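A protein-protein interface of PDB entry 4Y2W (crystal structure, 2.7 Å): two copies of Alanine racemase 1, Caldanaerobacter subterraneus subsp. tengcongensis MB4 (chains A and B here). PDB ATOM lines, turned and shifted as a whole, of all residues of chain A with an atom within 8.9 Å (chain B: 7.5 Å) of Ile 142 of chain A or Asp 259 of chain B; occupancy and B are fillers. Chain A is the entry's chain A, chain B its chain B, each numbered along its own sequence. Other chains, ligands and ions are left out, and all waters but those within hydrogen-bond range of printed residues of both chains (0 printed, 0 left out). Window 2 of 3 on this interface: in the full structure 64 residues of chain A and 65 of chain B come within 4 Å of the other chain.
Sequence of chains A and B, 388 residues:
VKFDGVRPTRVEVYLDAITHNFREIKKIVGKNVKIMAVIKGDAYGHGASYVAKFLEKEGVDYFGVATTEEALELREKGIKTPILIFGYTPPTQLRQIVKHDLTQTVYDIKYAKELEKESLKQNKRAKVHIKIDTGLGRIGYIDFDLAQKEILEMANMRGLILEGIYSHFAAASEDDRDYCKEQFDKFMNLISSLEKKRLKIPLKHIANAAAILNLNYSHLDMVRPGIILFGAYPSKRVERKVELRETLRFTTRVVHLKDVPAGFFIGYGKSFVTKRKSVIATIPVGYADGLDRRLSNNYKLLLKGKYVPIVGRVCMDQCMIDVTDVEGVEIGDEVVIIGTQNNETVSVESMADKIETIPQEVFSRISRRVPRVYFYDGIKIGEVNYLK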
ATOM      1  N   TYR A 107     -29.675   8.722   3.376  1.00  0.00           N
ATOM      2  CA  TYR A 107     -28.812   8.117   2.360  1.00  0.00           C
ATOM      3  C   TYR A 107     -27.356   7.958   2.830  1.00  0.00           C
ATOM      4  O   TYR A 107     -26.425   8.044   2.030  1.00  0.00           O
ATOM      5  CB  TYR A 107     -28.886   8.915   1.047  1.00  0.00           C
ATOM      6  CG  TYR A 107     -28.660  10.404   1.207  1.00  0.00           C
ATOM      7  CD1 TYR A 107     -27.381  10.948   1.148  1.00  0.00           C
ATOM      8  CD2 TYR A 107     -29.731  11.271   1.417  1.00  0.00           C
ATOM      9  CE1 TYR A 107     -27.176  12.309   1.295  1.00  0.00           C
ATOM     10  CE2 TYR A 107     -29.534  12.633   1.566  1.00  0.00           C
ATOM     11  CZ  TYR A 107     -28.255  13.147   1.504  1.00  0.00           C
ATOM     12  OH  TYR A 107     -28.052  14.497   1.651  1.00  0.00           O
ATOM     13  N   LYS A 131     -33.248   7.699  -0.158  1.00  0.00           N
ATOM     14  CA  LYS A 131     -33.149   8.406  -1.426  1.00  0.00           C
ATOM     15  C   LYS A 131     -32.048   7.863  -2.268  1.00  0.00           C
ATOM     16  O   LYS A 131     -30.947   7.675  -1.820  1.00  0.00           O
ATOM     17  CB  LYS A 131     -33.004   9.928  -1.270  1.00  0.00           C
ATOM     18  CG  LYS A 131     -32.516  10.687  -2.502  1.00  0.00           C
ATOM     19  CD  LYS A 131     -33.586  11.360  -3.354  1.00  0.00           C
ATOM     20  CE  LYS A 131     -32.996  12.184  -4.504  1.00  0.00           C
ATOM     21  NZ  LYS A 131     -33.259  13.655  -4.599  1.00  0.00           N
ATOM     22  N   ILE A 132     -32.379   7.630  -3.523  1.00  0.00           N
ATOM     23  CA  ILE A 132     -31.437   7.124  -4.479  1.00  0.00           C
ATOM     24  C   ILE A 132     -31.168   8.136  -5.574  1.00  0.00           C
ATOM     25  O   ILE A 132     -32.070   8.702  -6.137  1.00  0.00           O
ATOM     26  CB  ILE A 132     -31.955   5.818  -5.092  1.00  0.00           C
ATOM     27  CG1 ILE A 132     -32.429   4.890  -3.998  1.00  0.00           C
ATOM     28  CG2 ILE A 132     -30.873   5.134  -5.883  1.00  0.00           C
ATOM     29  CD1 ILE A 132     -31.324   4.396  -3.104  1.00  0.00           C
ATOM     30  N   ASP A 133     -29.905   8.345  -5.880  1.00  0.00           N
ATOM     31  CA  ASP A 133     -29.532   9.263  -6.947  1.00  0.00           C
ATOM     32  C   ASP A 133     -29.351   8.483  -8.249  1.00  0.00           C
ATOM     33  O   ASP A 133     -28.327   7.829  -8.456  1.00  0.00           O
ATOM     34  CB  ASP A 133     -28.248  10.000  -6.571  1.00  0.00           C
ATOM     35  CG  ASP A 133     -28.014  11.233  -7.413  1.00  0.00           C
ATOM     36  OD1 ASP A 133     -28.400  11.234  -8.605  1.00  0.00           O
ATOM     37  OD2 ASP A 133     -27.436  12.206  -6.875  1.00  0.00           O
ATOM     38  N   THR A 134     -30.350   8.556  -9.123  1.00  0.00           N
ATOM     39  CA  THR A 134     -30.349   7.798 -10.371  1.00  0.00           C
ATOM     40  C   THR A 134     -29.891   8.618 -11.577  1.00  0.00           C
ATOM     41  O   THR A 134     -29.934   8.123 -12.702  1.00  0.00           O
ATOM     42  CB  THR A 134     -31.751   7.227 -10.668  1.00  0.00           C
ATOM     43  OG1 THR A 134     -32.725   8.275 -10.610  1.00  0.00           O
ATOM     44  CG2 THR A 134     -32.117   6.154  -9.658  1.00  0.00           C
ATOM     45  N   GLY A 135     -29.437   9.851 -11.353  1.00  0.00           N
ATOM     46  CA  GLY A 135     -29.009  10.726 -12.457  1.00  0.00           C
ATOM     47  C   GLY A 135     -28.972  12.220 -12.159  1.00  0.00           C
ATOM     48  O   GLY A 135     -28.146  12.947 -12.721  1.00  0.00           O
ATOM     49  N   LEU A 136     -29.868  12.674 -11.281  1.00  0.00           N
ATOM     50  CA  LEU A 136     -30.010  14.094 -10.945  1.00  0.00           C
ATOM     51  C   LEU A 136     -28.769  14.719 -10.281  1.00  0.00           C
ATOM     52  O   LEU A 136     -28.557  15.933 -10.374  1.00  0.00           O
ATOM     53  CB  LEU A 136     -31.241  14.282 -10.046  1.00  0.00           C
ATOM     54  CG  LEU A 136     -31.646  15.694  -9.609  1.00  0.00           C
ATOM     55  CD1 LEU A 136     -32.043  16.568 -10.790  1.00  0.00           C
ATOM     56  CD2 LEU A 136     -32.786  15.613  -8.604  1.00  0.00           C
ATOM     57  N   GLY A 137     -27.958  13.899  -9.614  1.00  0.00           N
ATOM     58  CA  GLY A 137     -26.715  14.367  -8.989  1.00  0.00           C
ATOM     59  C   GLY A 137     -26.908  15.291  -7.794  1.00  0.00           C
ATOM     60  O   GLY A 137     -25.994  16.029  -7.427  1.00  0.00           O
ATOM     61  N   ARG A 138     -28.085  15.237  -7.173  1.00  0.00           N
ATOM     62  CA  ARG A 138     -28.454  16.177  -6.117  1.00  0.00           C
ATOM     63  C   ARG A 138     -28.234  15.560  -4.729  1.00  0.00           C
ATOM     64  O   ARG A 138     -27.238  15.877  -4.073  1.00  0.00           O
ATOM     65  CB  ARG A 138     -29.895  16.645  -6.330  1.00  0.00           C
ATOM     66  CG  ARG A 138     -30.391  17.698  -5.358  1.00  0.00           C
ATOM     67  CD  ARG A 138     -31.740  18.240  -5.809  1.00  0.00           C
ATOM     68  NE  ARG A 138     -32.839  17.316  -5.533  1.00  0.00           N
ATOM     69  CZ  ARG A 138     -34.115  17.547  -5.832  1.00  0.00           C
ATOM     70  NH1 ARG A 138     -34.479  18.678  -6.427  1.00  0.00           N
ATOM     71  NH2 ARG A 138     -35.036  16.638  -5.542  1.00  0.00           N
ATOM     72  N   ILE A 139     -29.143  14.691  -4.279  1.00  0.00           N
ATOM     73  CA  ILE A 139     -28.911  13.903  -3.061  1.00  0.00           C
ATOM     74  C   ILE A 139     -29.274  12.439  -3.280  1.00  0.00           C
ATOM     75  O   ILE A 139     -30.021  12.105  -4.203  1.00  0.00           O
ATOM     76  CB  ILE A 139     -29.677  14.440  -1.821  1.00  0.00           C
ATOM     77  CG1 ILE A 139     -31.184  14.520  -2.076  1.00  0.00           C
ATOM     78  CG2 ILE A 139     -29.139  15.798  -1.402  1.00  0.00           C
ATOM     79  CD1 ILE A 139     -32.010  14.467  -0.806  1.00  0.00           C
ATOM     80  N   GLY A 140     -28.741  11.581  -2.413  1.00  0.00           N
ATOM     81  CA  GLY A 140     -28.989  10.145  -2.465  1.00  0.00           C
ATOM     82  C   GLY A 140     -27.725   9.371  -2.770  1.00  0.00           C
ATOM     83  O   GLY A 140     -26.693   9.953  -3.109  1.00  0.00           O
ATOM     84  N   TYR A 141     -27.809   8.050  -2.646  1.00  0.00           N
ATOM     85  CA  TYR A 141     -26.686   7.174  -2.973  1.00  0.00           C
ATOM     86  C   TYR A 141     -26.364   7.227  -4.460  1.00  0.00           C
ATOM     87  O   TYR A 141     -27.270   7.220  -5.296  1.00  0.00           O
ATOM     88  CB  TYR A 141     -27.007   5.725  -2.606  1.00  0.00           C
ATOM     89  CG  TYR A 141     -27.008   5.438  -1.130  1.00  0.00           C
ATOM     90  CD1 TYR A 141     -25.814   5.363  -0.420  1.00  0.00           C
ATOM     91  CD2 TYR A 141     -28.201   5.216  -0.445  1.00  0.00           C
ATOM     92  CE1 TYR A 141     -25.807   5.088   0.935  1.00  0.00           C
ATOM     93  CE2 TYR A 141     -28.206   4.939   0.911  1.00  0.00           C
ATOM     94  CZ  TYR A 141     -27.009   4.876   1.598  1.00  0.00           C
ATOM     95  OH  TYR A 141     -27.017   4.600   2.946  1.00  0.00           O
ATOM     96  N   ILE A 142     -25.074   7.275  -4.778  1.00  0.00           N
ATOM     97  CA  ILE A 142     -24.606   7.114  -6.158  1.00  0.00           C
ATOM     98  C   ILE A 142     -23.879   5.778  -6.353  1.00  0.00           C
ATOM     99  O   ILE A 142     -23.976   5.175  -7.423  1.00  0.00           O
ATOM    100  CB  ILE A 142     -23.722   8.295  -6.639  1.00  0.00           C
ATOM    101  CG1 ILE A 142     -22.556   8.564  -5.678  1.00  0.00           C
ATOM    102  CG2 ILE A 142     -24.572   9.547  -6.805  1.00  0.00           C
ATOM    103  CD1 ILE A 142     -21.480   9.453  -6.264  1.00  0.00           C
ATOM    104  N   ASP A 143     -23.157   5.326  -5.325  1.00  0.00           N
ATOM    105  CA  ASP A 143     -22.549   3.997  -5.313  1.00  0.00           C
ATOM    106  C   ASP A 143     -23.627   2.997  -4.895  1.00  0.00           C
ATOM    107  O   ASP A 143     -23.953   2.883  -3.713  1.00  0.00           O
ATOM    108  CB  ASP A 143     -21.359   3.973  -4.344  1.00  0.00           C
ATOM    109  CG  ASP A 143     -20.629   2.634  -4.318  1.00  0.00           C
ATOM    110  OD1 ASP A 143     -21.146   1.633  -4.857  1.00  0.00           O
ATOM    111  OD2 ASP A 143     -19.526   2.582  -3.737  1.00  0.00           O
ATOM    112  N   PHE A 144     -24.183   2.286  -5.873  1.00  0.00           N
ATOM    113  CA  PHE A 144     -25.295   1.353  -5.637  1.00  0.00           C
ATOM    114  C   PHE A 144     -24.847   0.127  -4.843  1.00  0.00           C
ATOM    115  O   PHE A 144     -25.645  -0.495  -4.139  1.00  0.00           O
ATOM    116  CB  PHE A 144     -25.913   0.910  -6.969  1.00  0.00           C
ATOM    117  CG  PHE A 144     -26.843   1.927  -7.586  1.00  0.00           C
ATOM    118  CD1 PHE A 144     -26.628   3.296  -7.436  1.00  0.00           C
ATOM    119  CD2 PHE A 144     -27.930   1.509  -8.342  1.00  0.00           C
ATOM    120  CE1 PHE A 144     -27.485   4.219  -8.012  1.00  0.00           C
ATOM    121  CE2 PHE A 144     -28.790   2.430  -8.920  1.00  0.00           C
ATOM    122  CZ  PHE A 144     -28.566   3.786  -8.756  1.00  0.00           C
ATOM    123  N   ASP A 145     -23.566  -0.209  -4.969  1.00  0.00           N
ATOM    124  CA  ASP A 145     -22.962  -1.318  -4.234  1.00  0.00           C
ATOM    125  C   ASP A 145     -22.926  -1.004  -2.734  1.00  0.00           C
ATOM    126  O   ASP A 145     -23.311  -1.826  -1.904  1.00  0.00           O
ATOM    127  CB  ASP A 145     -21.545  -1.570  -4.766  1.00  0.00           C
ATOM    128  CG  ASP A 145     -21.056  -2.971  -4.491  1.00  0.00           C
ATOM    129  OD1 ASP A 145     -21.773  -3.930  -4.838  1.00  0.00           O
ATOM    130  OD2 ASP A 145     -19.941  -3.113  -3.945  1.00  0.00           O
ATOM    131  N   LEU A 146     -22.466   0.201  -2.409  1.00  0.00           N
ATOM    132  CA  LEU A 146     -22.491   0.717  -1.044  1.00  0.00           C
ATOM    133  C   LEU A 146     -23.919   0.845  -0.518  1.00  0.00           C
ATOM    134  O   LEU A 146     -24.184   0.574   0.653  1.00  0.00           O
ATOM    135  CB  LEU A 146     -21.812   2.089  -0.995  1.00  0.00           C
ATOM    136  CG  LEU A 146     -21.892   2.870   0.321  1.00  0.00           C
ATOM    137  CD1 LEU A 146     -21.248   2.079   1.449  1.00  0.00           C
ATOM    138  CD2 LEU A 146     -21.238   4.237   0.171  1.00  0.00           C
ATOM    139  N   ALA A 147     -24.826   1.280  -1.388  1.00  0.00           N
ATOM    140  CA  ALA A 147     -26.221   1.487  -1.015  1.00  0.00           C
ATOM    141  C   ALA A 147     -26.855   0.206  -0.487  1.00  0.00           C
ATOM    142  O   ALA A 147     -27.481   0.216   0.570  1.00  0.00           O
ATOM    143  CB  ALA A 147     -27.013   2.021  -2.199  1.00  0.00           C
ATOM    144  N   GLN A 148     -26.684  -0.893  -1.218  1.00  0.00           N
ATOM    145  CA  GLN A 148     -27.244  -2.186  -0.809  1.00  0.00           C
ATOM    146  C   GLN A 148     -26.778  -2.590   0.582  1.00  0.00           C
ATOM    147  O   GLN A 148     -27.583  -3.022   1.404  1.00  0.00           O
ATOM    148  CB  GLN A 148     -26.864  -3.291  -1.797  1.00  0.00           C
ATOM    149  CG  GLN A 148     -27.574  -3.200  -3.136  1.00  0.00           C
ATOM    150  CD  GLN A 148     -27.273  -4.381  -4.041  1.00  0.00           C
ATOM    151  OE1 GLN A 148     -26.932  -4.208  -5.214  1.00  0.00           O
ATOM    152  NE2 GLN A 148     -27.403  -5.590  -3.502  1.00  0.00           N
ATOM    153  N   LYS A 186     -32.338   1.812 -13.584  1.00  0.00           N
ATOM    154  CA  LYS A 186     -31.321   1.808 -12.522  1.00  0.00           C
ATOM    155  C   LYS A 186     -31.961   1.642 -11.152  1.00  0.00           C
ATOM    156  O   LYS A 186     -31.501   0.847 -10.331  1.00  0.00           O
ATOM    157  CB  LYS A 186     -30.518   3.106 -12.524  1.00  0.00           C
ATOM    158  CG  LYS A 186     -29.475   3.203 -13.620  1.00  0.00           C
ATOM    159  CD  LYS A 186     -28.521   4.352 -13.343  1.00  0.00           C
ATOM    160  CE  LYS A 186     -27.570   4.581 -14.504  1.00  0.00           C
ATOM    161  NZ  LYS A 186     -26.639   5.711 -14.238  1.00  0.00           N
ATOM    162  N   LEU A 190     -31.676  -1.645  -8.540  1.00  0.00           N
ATOM    163  CA  LEU A 190     -31.258  -1.620  -7.143  1.00  0.00           C
ATOM    164  C   LEU A 190     -32.292  -2.310  -6.250  1.00  0.00           C
ATOM    165  O   LEU A 190     -31.928  -2.955  -5.269  1.00  0.00           O
ATOM    166  CB  LEU A 190     -31.034  -0.185  -6.665  1.00  0.00           C
ATOM    167  CG  LEU A 190     -30.454  -0.023  -5.255  1.00  0.00           C
ATOM    168  CD1 LEU A 190     -29.092  -0.693  -5.147  1.00  0.00           C
ATOM    169  CD2 LEU A 190     -30.354   1.449  -4.885  1.00  0.00           C
ATOM    170  N   HIS B 256     -24.579  17.601   1.904  1.00  0.00           N
ATOM    171  CA  HIS B 256     -24.063  16.371   1.302  1.00  0.00           C
ATOM    172  C   HIS B 256     -22.777  16.639   0.541  1.00  0.00           C
ATOM    173  O   HIS B 256     -22.639  17.674  -0.102  1.00  0.00           O
ATOM    174  CB  HIS B 256     -25.103  15.765   0.362  1.00  0.00           C
ATOM    175  CG  HIS B 256     -24.724  14.423  -0.187  1.00  0.00           C
ATOM    176  ND1 HIS B 256     -24.072  13.463   0.560  1.00  0.00           N
ATOM    177  CD2 HIS B 256     -24.935  13.870  -1.406  1.00  0.00           C
ATOM    178  CE1 HIS B 256     -23.888  12.383  -0.179  1.00  0.00           C
ATOM    179  NE2 HIS B 256     -24.401  12.605  -1.377  1.00  0.00           N
ATOM    180  N   LEU B 257     -21.837  15.705   0.645  1.00  0.00           N
ATOM    181  CA  LEU B 257     -20.609  15.721  -0.139  1.00  0.00           C
ATOM    182  C   LEU B 257     -20.522  14.415  -0.904  1.00  0.00           C
ATOM    183  O   LEU B 257     -20.971  13.378  -0.418  1.00  0.00           O
ATOM    184  CB  LEU B 257     -19.388  15.850   0.772  1.00  0.00           C
ATOM    185  CG  LEU B 257     -19.133  17.220   1.402  1.00  0.00           C
ATOM    186  CD1 LEU B 257     -18.205  17.094   2.601  1.00  0.00           C
ATOM    187  CD2 LEU B 257     -18.559  18.193   0.381  1.00  0.00           C
ATOM    188  N   LYS B 258     -19.948  14.462  -2.101  1.00  0.00           N
ATOM    189  CA  LYS B 258     -19.696  13.250  -2.865  1.00  0.00           C
ATOM    190  C   LYS B 258     -18.583  13.453  -3.881  1.00  0.00           C
ATOM    191  O   LYS B 258     -18.432  14.542  -4.437  1.00  0.00           O
ATOM    192  CB  LYS B 258     -20.973  12.779  -3.567  1.00  0.00           C
ATOM    193  CG  LYS B 258     -21.606  13.789  -4.513  1.00  0.00           C
ATOM    194  CD  LYS B 258     -22.744  13.160  -5.309  1.00  0.00           C
ATOM    195  CE  LYS B 258     -23.592  14.206  -6.011  1.00  0.00           C
ATOM    196  NZ  LYS B 258     -24.407  15.013  -5.058  1.00  0.00           N
ATOM    197  N   ASP B 259     -17.799  12.401  -4.104  1.00  0.00           N
ATOM    198  CA  ASP B 259     -16.823  12.379  -5.184  1.00  0.00           C
ATOM    199  C   ASP B 259     -17.529  11.873  -6.435  1.00  0.00           C
ATOM    200  O   ASP B 259     -18.306  10.909  -6.372  1.00  0.00           O
ATOM    201  CB  ASP B 259     -15.640  11.472  -4.837  1.00  0.00           C
ATOM    202  CG  ASP B 259     -14.884  11.935  -3.599  1.00  0.00           C
ATOM    203  OD1 ASP B 259     -14.593  13.145  -3.485  1.00  0.00           O
ATOM    204  OD2 ASP B 259     -14.580  11.086  -2.735  1.00  0.00           O
ATOM    205  N   VAL B 260     -17.282  12.539  -7.561  1.00  0.00           N
ATOM    206  CA  VAL B 260     -17.839  12.125  -8.843  1.00  0.00           C
ATOM    207  C   VAL B 260     -16.774  12.211  -9.933  1.00  0.00           C
ATOM    208  O   VAL B 260     -15.897  13.078  -9.878  1.00  0.00           O
ATOM    209  CB  VAL B 260     -19.070  12.972  -9.253  1.00  0.00           C
ATOM    210  CG1 VAL B 260     -20.190  12.820  -8.235  1.00  0.00           C
ATOM    211  CG2 VAL B 260     -18.703  14.441  -9.436  1.00  0.00           C
ATOM    212  N   PRO B 261     -16.848  11.317 -10.934  1.00  0.00           N
ATOM    213  CA  PRO B 261     -15.895  11.356 -12.034  1.00  0.00           C
ATOM    214  C   PRO B 261     -16.253  12.444 -13.047  1.00  0.00           C
ATOM    215  O   PRO B 261     -17.209  13.200 -12.838  1.00  0.00           O
ATOM    216  CB  PRO B 261     -16.054   9.972 -12.661  1.00  0.00           C
ATOM    217  CG  PRO B 261     -17.496   9.656 -12.455  1.00  0.00           C
ATOM    218  CD  PRO B 261     -17.871  10.272 -11.137  1.00  0.00           C
ATOM    219  N   PHE B 264     -20.115  13.571 -15.322  1.00  0.00           N
ATOM    220  CA  PHE B 264     -21.190  13.403 -14.347  1.00  0.00           C
ATOM    221  C   PHE B 264     -22.171  14.567 -14.438  1.00  0.00           C
ATOM    222  O   PHE B 264     -21.833  15.702 -14.085  1.00  0.00           O
ATOM    223  CB  PHE B 264     -20.621  13.318 -12.929  1.00  0.00           C
ATOM    224  CG  PHE B 264     -21.653  13.010 -11.881  1.00  0.00           C
ATOM    225  CD1 PHE B 264     -22.372  14.031 -11.271  1.00  0.00           C
ATOM    226  CD2 PHE B 264     -21.909  11.698 -11.504  1.00  0.00           C
ATOM    227  CE1 PHE B 264     -23.326  13.750 -10.304  1.00  0.00           C
ATOM    228  CE2 PHE B 264     -22.860  11.411 -10.538  1.00  0.00           C
ATOM    229  CZ  PHE B 264     -23.571  12.438  -9.938  1.00  0.00           C
ATOM    230  N   LYS B 277     -12.545  14.806 -12.529  1.00  0.00           N
ATOM    231  CA  LYS B 277     -12.967  14.154 -11.295  1.00  0.00           C
ATOM    232  C   LYS B 277     -13.210  15.268 -10.280  1.00  0.00           C
ATOM    233  O   LYS B 277     -12.320  16.085 -10.030  1.00  0.00           O
ATOM    234  CB  LYS B 277     -11.921  13.153 -10.786  1.00  0.00           C
ATOM    235  CG  LYS B 277     -12.551  11.955 -10.087  1.00  0.00           C
ATOM    236  CD  LYS B 277     -11.578  11.194  -9.201  1.00  0.00           C
ATOM    237  CE  LYS B 277     -12.301  10.093  -8.432  1.00  0.00           C
ATOM    238  NZ  LYS B 277     -11.496   9.537  -7.308  1.00  0.00           N
ATOM    239  N   SER B 278     -14.422  15.313  -9.723  1.00  0.00           N
ATOM    240  CA  SER B 278     -14.866  16.446  -8.909  1.00  0.00           C
ATOM    241  C   SER B 278     -15.461  16.033  -7.570  1.00  0.00           C
ATOM    242  O   SER B 278     -15.969  14.924  -7.412  1.00  0.00           O
ATOM    243  CB  SER B 278     -15.906  17.263  -9.675  1.00  0.00           C
ATOM    244  OG  SER B 278     -15.372  17.753 -10.889  1.00  0.00           O
ATOM    245  N   VAL B 279     -15.383  16.951  -6.612  1.00  0.00           N
ATOM    246  CA  VAL B 279     -16.047  16.812  -5.326  1.00  0.00           C
ATOM    247  C   VAL B 279     -17.177  17.836  -5.312  1.00  0.00           C
ATOM    248  O   VAL B 279     -16.928  19.039  -5.390  1.00  0.00           O
ATOM    249  CB  VAL B 279     -15.085  17.079  -4.149  1.00  0.00           C
ATOM    250  CG1 VAL B 279     -15.734  16.682  -2.829  1.00  0.00           C
ATOM    251  CG2 VAL B 279     -13.772  16.332  -4.347  1.00  0.00           C
ATOM    252  N   ILE B 280     -18.415  17.354  -5.231  1.00  0.00           N
ATOM    253  CA  ILE B 280     -19.591  18.216  -5.303  1.00  0.00           C
ATOM    254  C   ILE B 280     -20.343  18.206  -3.973  1.00  0.00           C
ATOM    255  O   ILE B 280     -20.559  17.144  -3.381  1.00  0.00           O
ATOM    256  CB  ILE B 280     -20.546  17.763  -6.430  1.00  0.00           C
ATOM    257  CG1 ILE B 280     -19.790  17.583  -7.753  1.00  0.00           C
ATOM    258  CG2 ILE B 280     -21.693  18.753  -6.598  1.00  0.00           C
ATOM    259  CD1 ILE B 280     -19.091  18.829  -8.259  1.00  0.00           C
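The side-chain amino group (NZ) of Lys 258 of chain B is in hydrogen-bond range of the backbone carbonyl oxygen (O) of Gly 137 of chain A (3.0 Å). The backbone carbonyl oxygen (O) of Arg 138 of chain A is in hydrogen-bond range of the side-chain amino group (NZ) of Lys 258 of chain B (3.1 Å).
OD1 of Asp 133 of chain A lies within hydrogen-bond range of N of Gly 137 of chain A (2.9 Å). The side-chain carboxylate (OD2) of Asp 133 of chain A is in hydrogen-bond range of the backbone NH (N) of Arg 138 of chain A (3.1 Å). O of Lys 258 of chain B lies within hydrogen-bond range of N of Ile 280 of chain B.
CE1 of Tyr 107 of chain A touches ND1 of His 256 of chain B, at 3.4 Å. Gly 137 of chain A touches Phe 264 of chain B (CA to CE1, 3.7 Å). NE2 of His 256 of chain B touches O of Gly 140 of chain A (3.9 Å). Ile 142 of chain A touches Asp 259 of chain B (CD1 to O, 3.5 Å).
Ile 142 of chain A touches just one residue of chain B: Asp 259 (3.5 Å). Of chain A, only Ile 142 comes within 4 Å of Asp 259 of chain B. No residue of chain A comes within 4 Å of Val 260 of chain B. Of the printed residues of chain A, Phe 264 of chain B touches Gly 137 (3.7 Å). Printed residues of chain B within 4 Å of Gly 137 of chain A: Lys 258 (3.0 Å) and Phe 264 (3.7 Å). Of the printed residues of chain A, His 256 of chain B touches Tyr 107 and Gly 140. The nearest residue of chain A that does not touch Asp 259 of chain B is Asp 143 of chain A (7.5 Å). The nearest printed residue of chain B that does not touch Tyr 107 of chain A is Leu 257 of chain B (6.4 Å).
Of the 21 printed residues of chain A, 5 touch a printed residue of chain B. Printed residues of chain A that touch a printed residue of chain B: Tyr 107, Gly 137, Arg 138, Gly 140 and Ile 142. Hydrophobic or aromatic side chains of chain B within 4 Å of the printed part of chain A: His 256 and Phe 264. Among the printed residues, 6 pairs touch across the chains.
No position is printed for both chains. Of the 6 pairs that touch across the chains among the printed residues, none has its exchanged pair printed and touching as well.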
